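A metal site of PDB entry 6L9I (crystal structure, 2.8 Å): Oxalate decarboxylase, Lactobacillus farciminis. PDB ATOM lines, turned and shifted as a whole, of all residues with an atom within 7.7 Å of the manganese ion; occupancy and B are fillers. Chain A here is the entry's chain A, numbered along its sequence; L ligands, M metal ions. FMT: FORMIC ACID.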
ATOM      1  N   MET A  63      38.071  25.075  23.373  1.00  0.00           N
ATOM      2  CA  MET A  63      37.994  26.347  22.654  1.00  0.00           C
ATOM      3  C   MET A  63      38.628  27.455  23.480  1.00  0.00           C
ATOM      4  O   MET A  63      38.559  27.461  24.709  1.00  0.00           O
ATOM      5  CB  MET A  63      36.533  26.711  22.319  1.00  0.00           C
ATOM      6  CG  MET A  63      36.391  27.851  21.333  1.00  0.00           C
ATOM      7  SD  MET A  63      34.695  28.011  20.748  1.00  0.00           S
ATOM      8  CE  MET A  63      34.541  26.512  19.770  1.00  0.00           C
ATOM      9  N   ARG A  71      32.537  33.760  19.583  1.00  0.00           N
ATOM     10  CA  ARG A  71      32.199  32.527  18.874  1.00  0.00           C
ATOM     11  C   ARG A  71      30.885  32.801  18.156  1.00  0.00           C
ATOM     12  O   ARG A  71      29.881  33.104  18.809  1.00  0.00           O
ATOM     13  CB  ARG A  71      32.078  31.321  19.807  1.00  0.00           C
ATOM     14  CG  ARG A  71      31.503  30.082  19.126  1.00  0.00           C
ATOM     15  CD  ARG A  71      32.428  29.542  18.032  1.00  0.00           C
ATOM     16  NE  ARG A  71      31.973  28.262  17.475  1.00  0.00           N
ATOM     17  CZ  ARG A  71      31.106  28.140  16.482  1.00  0.00           C
ATOM     18  NH1 ARG A  71      30.589  29.220  15.919  1.00  0.00           N
ATOM     19  NH2 ARG A  71      30.748  26.934  16.046  1.00  0.00           N
ATOM     20  N   GLU A  72      30.905  32.747  16.830  1.00  0.00           N
ATOM     21  CA  GLU A  72      29.798  33.288  16.038  1.00  0.00           C
ATOM     22  C   GLU A  72      28.457  32.700  16.463  1.00  0.00           C
ATOM     23  O   GLU A  72      28.368  31.539  16.881  1.00  0.00           O
ATOM     24  CB  GLU A  72      30.027  33.023  14.554  1.00  0.00           C
ATOM     25  CG  GLU A  72      28.930  33.595  13.664  1.00  0.00           C
ATOM     26  CD  GLU A  72      29.022  33.138  12.234  1.00  0.00           C
ATOM     27  OE1 GLU A  72      30.085  32.620  11.837  1.00  0.00           O
ATOM     28  OE2 GLU A  72      28.018  33.288  11.507  1.00  0.00           O
ATOM     29  N   HIS A  74      25.289  30.801  16.330  1.00  0.00           N
ATOM     30  CA  HIS A  74      25.211  29.518  15.654  1.00  0.00           C
ATOM     31  C   HIS A  74      24.235  28.609  16.384  1.00  0.00           C
ATOM     32  O   HIS A  74      23.720  28.944  17.455  1.00  0.00           O
ATOM     33  CB  HIS A  74      26.586  28.866  15.566  1.00  0.00           C
ATOM     34  CG  HIS A  74      27.104  28.406  16.898  1.00  0.00           C
ATOM     35  ND1 HIS A  74      27.909  29.187  17.687  1.00  0.00           N
ATOM     36  CD2 HIS A  74      26.907  27.246  17.571  1.00  0.00           C
ATOM     37  CE1 HIS A  74      28.202  28.527  18.795  1.00  0.00           C
ATOM     38  NE2 HIS A  74      27.595  27.354  18.755  1.00  0.00           N
ATOM     39  N   TRP A  75      23.998  27.441  15.796  1.00  0.00           N
ATOM     40  CA  TRP A  75      23.188  26.410  16.429  1.00  0.00           C
ATOM     41  C   TRP A  75      23.605  25.056  15.862  1.00  0.00           C
ATOM     42  O   TRP A  75      24.347  24.971  14.885  1.00  0.00           O
ATOM     43  CB  TRP A  75      21.688  26.679  16.243  1.00  0.00           C
ATOM     44  CG  TRP A  75      21.095  26.354  14.887  1.00  0.00           C
ATOM     45  CD1 TRP A  75      20.472  25.204  14.517  1.00  0.00           C
ATOM     46  CD2 TRP A  75      21.027  27.231  13.745  1.00  0.00           C
ATOM     47  NE1 TRP A  75      20.036  25.297  13.216  1.00  0.00           N
ATOM     48  CE2 TRP A  75      20.366  26.526  12.721  1.00  0.00           C
ATOM     49  CE3 TRP A  75      21.471  28.528  13.487  1.00  0.00           C
ATOM     50  CZ2 TRP A  75      20.134  27.075  11.467  1.00  0.00           C
ATOM     51  CZ3 TRP A  75      21.239  29.077  12.233  1.00  0.00           C
ATOM     52  CH2 TRP A  75      20.578  28.348  11.236  1.00  0.00           C
ATOM     53  N   HIS A  76      23.119  23.987  16.511  1.00  0.00           N
ATOM     54  CA  HIS A  76      23.405  22.637  16.048  1.00  0.00           C
ATOM     55  C   HIS A  76      22.332  21.682  16.531  1.00  0.00           C
ATOM     56  O   HIS A  76      21.580  21.956  17.473  1.00  0.00           O
ATOM     57  CB  HIS A  76      24.784  22.155  16.520  1.00  0.00           C
ATOM     58  CG  HIS A  76      25.240  22.749  17.812  1.00  0.00           C
ATOM     59  ND1 HIS A  76      24.588  22.522  19.010  1.00  0.00           N
ATOM     60  CD2 HIS A  76      26.303  23.527  18.107  1.00  0.00           C
ATOM     61  CE1 HIS A  76      25.228  23.160  19.976  1.00  0.00           C
ATOM     62  NE2 HIS A  76      26.275  23.782  19.457  1.00  0.00           N
ATOM     63  N   GLU A  78      22.907  18.890  17.995  1.00  0.00           N
ATOM     64  CA  GLU A  78      23.303  18.239  19.232  1.00  0.00           C
ATOM     65  C   GLU A  78      23.129  19.184  20.409  1.00  0.00           C
ATOM     66  O   GLU A  78      23.141  20.409  20.263  1.00  0.00           O
ATOM     67  CB  GLU A  78      24.764  17.773  19.146  1.00  0.00           C
ATOM     68  CG  GLU A  78      25.021  16.709  18.104  1.00  0.00           C
ATOM     69  CD  GLU A  78      25.490  17.273  16.785  1.00  0.00           C
ATOM     70  OE1 GLU A  78      25.274  18.477  16.523  1.00  0.00           O
ATOM     71  OE2 GLU A  78      26.111  16.519  16.015  1.00  0.00           O
ATOM     72  N   ALA A  79      23.012  18.603  21.596  1.00  0.00           N
ATOM     73  CA  ALA A  79      22.998  19.419  22.792  1.00  0.00           C
ATOM     74  C   ALA A  79      24.427  19.593  23.302  1.00  0.00           C
ATOM     75  O   ALA A  79      25.234  18.670  23.267  1.00  0.00           O
ATOM     76  CB  ALA A  79      22.109  18.801  23.869  1.00  0.00           C
ATOM     77  N   GLU A  80      24.728  20.802  23.748  1.00  0.00           N
ATOM     78  CA  GLU A  80      26.071  21.101  24.222  1.00  0.00           C
ATOM     79  C   GLU A  80      26.088  21.422  25.704  1.00  0.00           C
ATOM     80  O   GLU A  80      25.203  22.116  26.225  1.00  0.00           O
ATOM     81  CB  GLU A  80      26.735  22.194  23.394  1.00  0.00           C
ATOM     82  CG  GLU A  80      26.373  23.622  23.637  1.00  0.00           C
ATOM     83  CD  GLU A  80      27.446  24.523  23.065  1.00  0.00           C
ATOM     84  OE1 GLU A  80      28.459  24.758  23.757  1.00  0.00           O
ATOM     85  OE2 GLU A  80      27.324  24.936  21.886  1.00  0.00           O
ATOM     86  N   TRP A 111      27.598  25.935  31.316  1.00  0.00           N
ATOM     87  CA  TRP A 111      26.386  26.277  30.599  1.00  0.00           C
ATOM     88  C   TRP A 111      25.865  25.047  29.853  1.00  0.00           C
ATOM     89  O   TRP A 111      26.542  24.030  29.756  1.00  0.00           O
ATOM     90  CB  TRP A 111      26.575  27.498  29.663  1.00  0.00           C
ATOM     91  CG  TRP A 111      27.378  27.330  28.393  1.00  0.00           C
ATOM     92  CD1 TRP A 111      27.001  26.660  27.268  1.00  0.00           C
ATOM     93  CD2 TRP A 111      28.636  27.937  28.084  1.00  0.00           C
ATOM     94  NE1 TRP A 111      27.972  26.771  26.296  1.00  0.00           N
ATOM     95  CE2 TRP A 111      28.984  27.562  26.773  1.00  0.00           C
ATOM     96  CE3 TRP A 111      29.531  28.735  28.803  1.00  0.00           C
ATOM     97  CZ2 TRP A 111      30.176  27.946  26.175  1.00  0.00           C
ATOM     98  CZ3 TRP A 111      30.705  29.132  28.200  1.00  0.00           C
ATOM     99  CH2 TRP A 111      31.022  28.740  26.896  1.00  0.00           C
ATOM    100  N   PHE A 113      23.090  24.127  26.460  1.00  0.00           N
ATOM    101  CA  PHE A 113      22.139  24.463  25.414  1.00  0.00           C
ATOM    102  C   PHE A 113      21.578  23.160  24.843  1.00  0.00           C
ATOM    103  O   PHE A 113      22.322  22.366  24.266  1.00  0.00           O
ATOM    104  CB  PHE A 113      22.803  25.300  24.325  1.00  0.00           C
ATOM    105  CG  PHE A 113      23.375  26.588  24.841  1.00  0.00           C
ATOM    106  CD1 PHE A 113      22.591  27.471  25.546  1.00  0.00           C
ATOM    107  CD2 PHE A 113      24.708  26.902  24.622  1.00  0.00           C
ATOM    108  CE1 PHE A 113      23.114  28.653  26.028  1.00  0.00           C
ATOM    109  CE2 PHE A 113      25.234  28.086  25.094  1.00  0.00           C
ATOM    110  CZ  PHE A 113      24.431  28.958  25.800  1.00  0.00           C
ATOM    111  N   ILE A 117      19.006  24.885  20.230  1.00  0.00           N
ATOM    112  CA  ILE A 117      18.875  26.121  20.901  1.00  0.00           C
ATOM    113  C   ILE A 117      20.027  27.098  20.388  1.00  0.00           C
ATOM    114  O   ILE A 117      21.186  26.718  20.624  1.00  0.00           O
ATOM    115  CB  ILE A 117      18.941  25.998  22.415  1.00  0.00           C
ATOM    116  CG1 ILE A 117      17.780  25.109  22.879  1.00  0.00           C
ATOM    117  CG2 ILE A 117      18.887  27.345  23.110  1.00  0.00           C
ATOM    118  CD1 ILE A 117      16.424  25.636  22.483  1.00  0.00           C
ATOM    119  N   PRO A 118      19.703  28.184  19.759  1.00  0.00           N
ATOM    120  CA  PRO A 118      20.787  29.054  19.271  1.00  0.00           C
ATOM    121  C   PRO A 118      21.369  29.872  20.402  1.00  0.00           C
ATOM    122  O   PRO A 118      20.691  30.280  21.350  1.00  0.00           O
ATOM    123  CB  PRO A 118      20.066  29.953  18.255  1.00  0.00           C
ATOM    124  CG  PRO A 118      18.695  30.100  18.837  1.00  0.00           C
ATOM    125  CD  PRO A 118      18.390  28.787  19.540  1.00  0.00           C
ATOM    126  N   HIS A 119      22.658  30.160  20.246  1.00  0.00           N
ATOM    127  CA  HIS A 119      23.425  30.796  21.305  1.00  0.00           C
ATOM    128  C   HIS A 119      24.681  31.433  20.728  1.00  0.00           C
ATOM    129  O   HIS A 119      25.079  31.138  19.599  1.00  0.00           O
ATOM    130  CB  HIS A 119      23.817  29.792  22.389  1.00  0.00           C
ATOM    131  CG  HIS A 119      24.459  28.551  21.849  1.00  0.00           C
ATOM    132  ND1 HIS A 119      23.720  27.490  21.368  1.00  0.00           N
ATOM    133  CD2 HIS A 119      25.751  28.199  21.703  1.00  0.00           C
ATOM    134  CE1 HIS A 119      24.533  26.546  20.934  1.00  0.00           C
ATOM    135  NE2 HIS A 119      25.777  26.948  21.130  1.00  0.00           N
ATOM    136  N   SER A 120      25.277  32.314  21.527  1.00  0.00           N
ATOM    137  CA  SER A 120      26.547  32.973  21.236  1.00  0.00           C
ATOM    138  C   SER A 120      27.401  33.046  22.498  1.00  0.00           C
ATOM    139  O   SER A 120      26.897  33.156  23.617  1.00  0.00           O
ATOM    140  CB  SER A 120      26.335  34.382  20.707  1.00  0.00           C
ATOM    141  OG  SER A 120      25.965  35.256  21.757  1.00  0.00           O
ATOM    142  N   ILE A 121      28.710  33.118  22.265  1.00  0.00           N
ATOM    143  CA  ILE A 121      29.710  33.255  23.324  1.00  0.00           C
ATOM    144  C   ILE A 121      30.640  34.391  22.952  1.00  0.00           C
ATOM    145  O   ILE A 121      31.068  34.480  21.797  1.00  0.00           O
ATOM    146  CB  ILE A 121      30.541  31.961  23.483  1.00  0.00           C
ATOM    147  CG1 ILE A 121      29.653  30.720  23.549  1.00  0.00           C
ATOM    148  CG2 ILE A 121      31.463  32.038  24.707  1.00  0.00           C
ATOM    149  CD1 ILE A 121      30.265  29.463  22.961  1.00  0.00           C
ATOM    150  N   PHE A 130      37.380  27.252  27.380  1.00  0.00           N
ATOM    151  CA  PHE A 130      36.315  26.415  27.895  1.00  0.00           C
ATOM    152  C   PHE A 130      36.251  25.108  27.120  1.00  0.00           C
ATOM    153  O   PHE A 130      36.663  25.005  25.956  1.00  0.00           O
ATOM    154  CB  PHE A 130      34.944  27.130  27.813  1.00  0.00           C
ATOM    155  CG  PHE A 130      34.691  27.841  26.503  1.00  0.00           C
ATOM    156  CD1 PHE A 130      35.067  29.166  26.325  1.00  0.00           C
ATOM    157  CD2 PHE A 130      34.054  27.184  25.456  1.00  0.00           C
ATOM    158  CE1 PHE A 130      34.820  29.819  25.135  1.00  0.00           C
ATOM    159  CE2 PHE A 130      33.799  27.833  24.262  1.00  0.00           C
ATOM    160  CZ  PHE A 130      34.184  29.152  24.097  1.00  0.00           C
ATOM    161  N   LEU A 132      33.643  22.205  25.781  1.00  0.00           N
ATOM    162  CA  LEU A 132      32.276  21.925  25.357  1.00  0.00           C
ATOM    163  C   LEU A 132      32.109  20.430  25.145  1.00  0.00           C
ATOM    164  O   LEU A 132      33.029  19.742  24.695  1.00  0.00           O
ATOM    165  CB  LEU A 132      31.935  22.666  24.065  1.00  0.00           C
ATOM    166  CG  LEU A 132      32.270  24.140  23.907  1.00  0.00           C
ATOM    167  CD1 LEU A 132      32.056  24.568  22.455  1.00  0.00           C
ATOM    168  CD2 LEU A 132      31.420  24.991  24.820  1.00  0.00           C
ATOM    169  N   PHE A 134      29.317  17.490  23.549  1.00  0.00           N
ATOM    170  CA  PHE A 134      28.197  17.374  22.625  1.00  0.00           C
ATOM    171  C   PHE A 134      27.630  15.969  22.654  1.00  0.00           C
ATOM    172  O   PHE A 134      28.377  14.986  22.746  1.00  0.00           O
ATOM    173  CB  PHE A 134      28.621  17.755  21.199  1.00  0.00           C
ATOM    174  CG  PHE A 134      29.047  19.187  21.077  1.00  0.00           C
ATOM    175  CD1 PHE A 134      30.351  19.561  21.378  1.00  0.00           C
ATOM    176  CD2 PHE A 134      28.140  20.170  20.692  1.00  0.00           C
ATOM    177  CE1 PHE A 134      30.743  20.881  21.293  1.00  0.00           C
ATOM    178  CE2 PHE A 134      28.532  21.490  20.607  1.00  0.00           C
ATOM    179  CZ  PHE A 134      29.838  21.842  20.903  1.00  0.00           C
ATOM    180  N   PHE A 139      30.157  14.514  16.389  1.00  0.00           N
ATOM    181  CA  PHE A 139      30.063  15.955  16.222  1.00  0.00           C
ATOM    182  C   PHE A 139      31.377  16.488  15.619  1.00  0.00           C
ATOM    183  O   PHE A 139      32.425  15.909  15.818  1.00  0.00           O
ATOM    184  CB  PHE A 139      29.800  16.559  17.611  1.00  0.00           C
ATOM    185  CG  PHE A 139      29.768  18.040  17.621  1.00  0.00           C
ATOM    186  CD1 PHE A 139      28.627  18.699  17.229  1.00  0.00           C
ATOM    187  CD2 PHE A 139      30.880  18.774  18.012  1.00  0.00           C
ATOM    188  CE1 PHE A 139      28.579  20.069  17.217  1.00  0.00           C
ATOM    189  CE2 PHE A 139      30.840  20.149  18.004  1.00  0.00           C
ATOM    190  CZ  PHE A 139      29.691  20.792  17.595  1.00  0.00           C
ATOM    191  N   GLU A 141      33.002  20.667  15.262  1.00  0.00           N
ATOM    192  CA  GLU A 141      32.804  22.103  15.251  1.00  0.00           C
ATOM    193  C   GLU A 141      32.750  22.698  13.847  1.00  0.00           C
ATOM    194  O   GLU A 141      32.244  23.806  13.691  1.00  0.00           O
ATOM    195  CB  GLU A 141      33.928  22.752  16.045  1.00  0.00           C
ATOM    196  CG  GLU A 141      33.550  23.060  17.482  1.00  0.00           C
ATOM    197  CD  GLU A 141      32.438  24.098  17.602  1.00  0.00           C
ATOM    198  OE1 GLU A 141      32.558  25.190  17.003  1.00  0.00           O
ATOM    199  OE2 GLU A 141      31.442  23.809  18.300  1.00  0.00           O
ATOM    200  N   THR A 144      28.813  23.177  12.118  1.00  0.00           N
ATOM    201  CA  THR A 144      27.778  23.837  12.890  1.00  0.00           C
ATOM    202  C   THR A 144      27.088  24.875  12.030  1.00  0.00           C
ATOM    203  O   THR A 144      27.643  25.373  11.047  1.00  0.00           O
ATOM    204  CB  THR A 144      28.375  24.489  14.140  1.00  0.00           C
ATOM    205  OG1 THR A 144      29.048  25.710  13.788  1.00  0.00           O
ATOM    206  CG2 THR A 144      29.349  23.545  14.837  1.00  0.00           C
HETATM  207  C   FMT L   1      29.710  25.580  19.878  1.00  0.00           C
HETATM  208  O1  FMT L   1      28.922  24.838  19.280  1.00  0.00           O
HETATM  209  O2  FMT L   1      30.785  25.953  19.396  1.00  0.00           O
HETATM  210 MN    MN M   1      27.622  25.808  20.455  1.00  0.00          MN
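O of Phe 113 lies within hydrogen-bond range of N of Glu 80, 2.9 Å away. The side-chain carboxylate (OE1) of Glu 80 lies within hydrogen-bond range of the indole nitrogen (NE1) of Trp 111. ND1 of His 119 is in hydrogen-bond range of O of Ile 117 (2.8 Å). ND1 of His 74 sits at hydrogen-bond distance from NH1 of Arg 71 (3.2 Å). A ring nitrogen (ND1) of His 74 lies within hydrogen-bond range of the backbone carbonyl oxygen of Glu 72, 2.5 Å away. ND1 of His 76 lies within hydrogen-bond range of O of Glu 78 (2.9 Å).
The manganese ion is bound by the side-chain carboxylate of Glu 80 (1.7 Å), an oxygen (O1) of the ligand (2.0 Å), a ring nitrogen (NE2) of His 119 (2.3 Å), a ring nitrogen (NE2) of His 74 (2.3 Å) and a ring nitrogen (NE2) of His 76 (2.6 Å).
Four residues have an atom within 4 Å of the manganese ion: His 74, His 76, Glu 80 and His 119. The nearest printed residue that does not touch the manganese ion is Phe 134 (4.4 Å).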
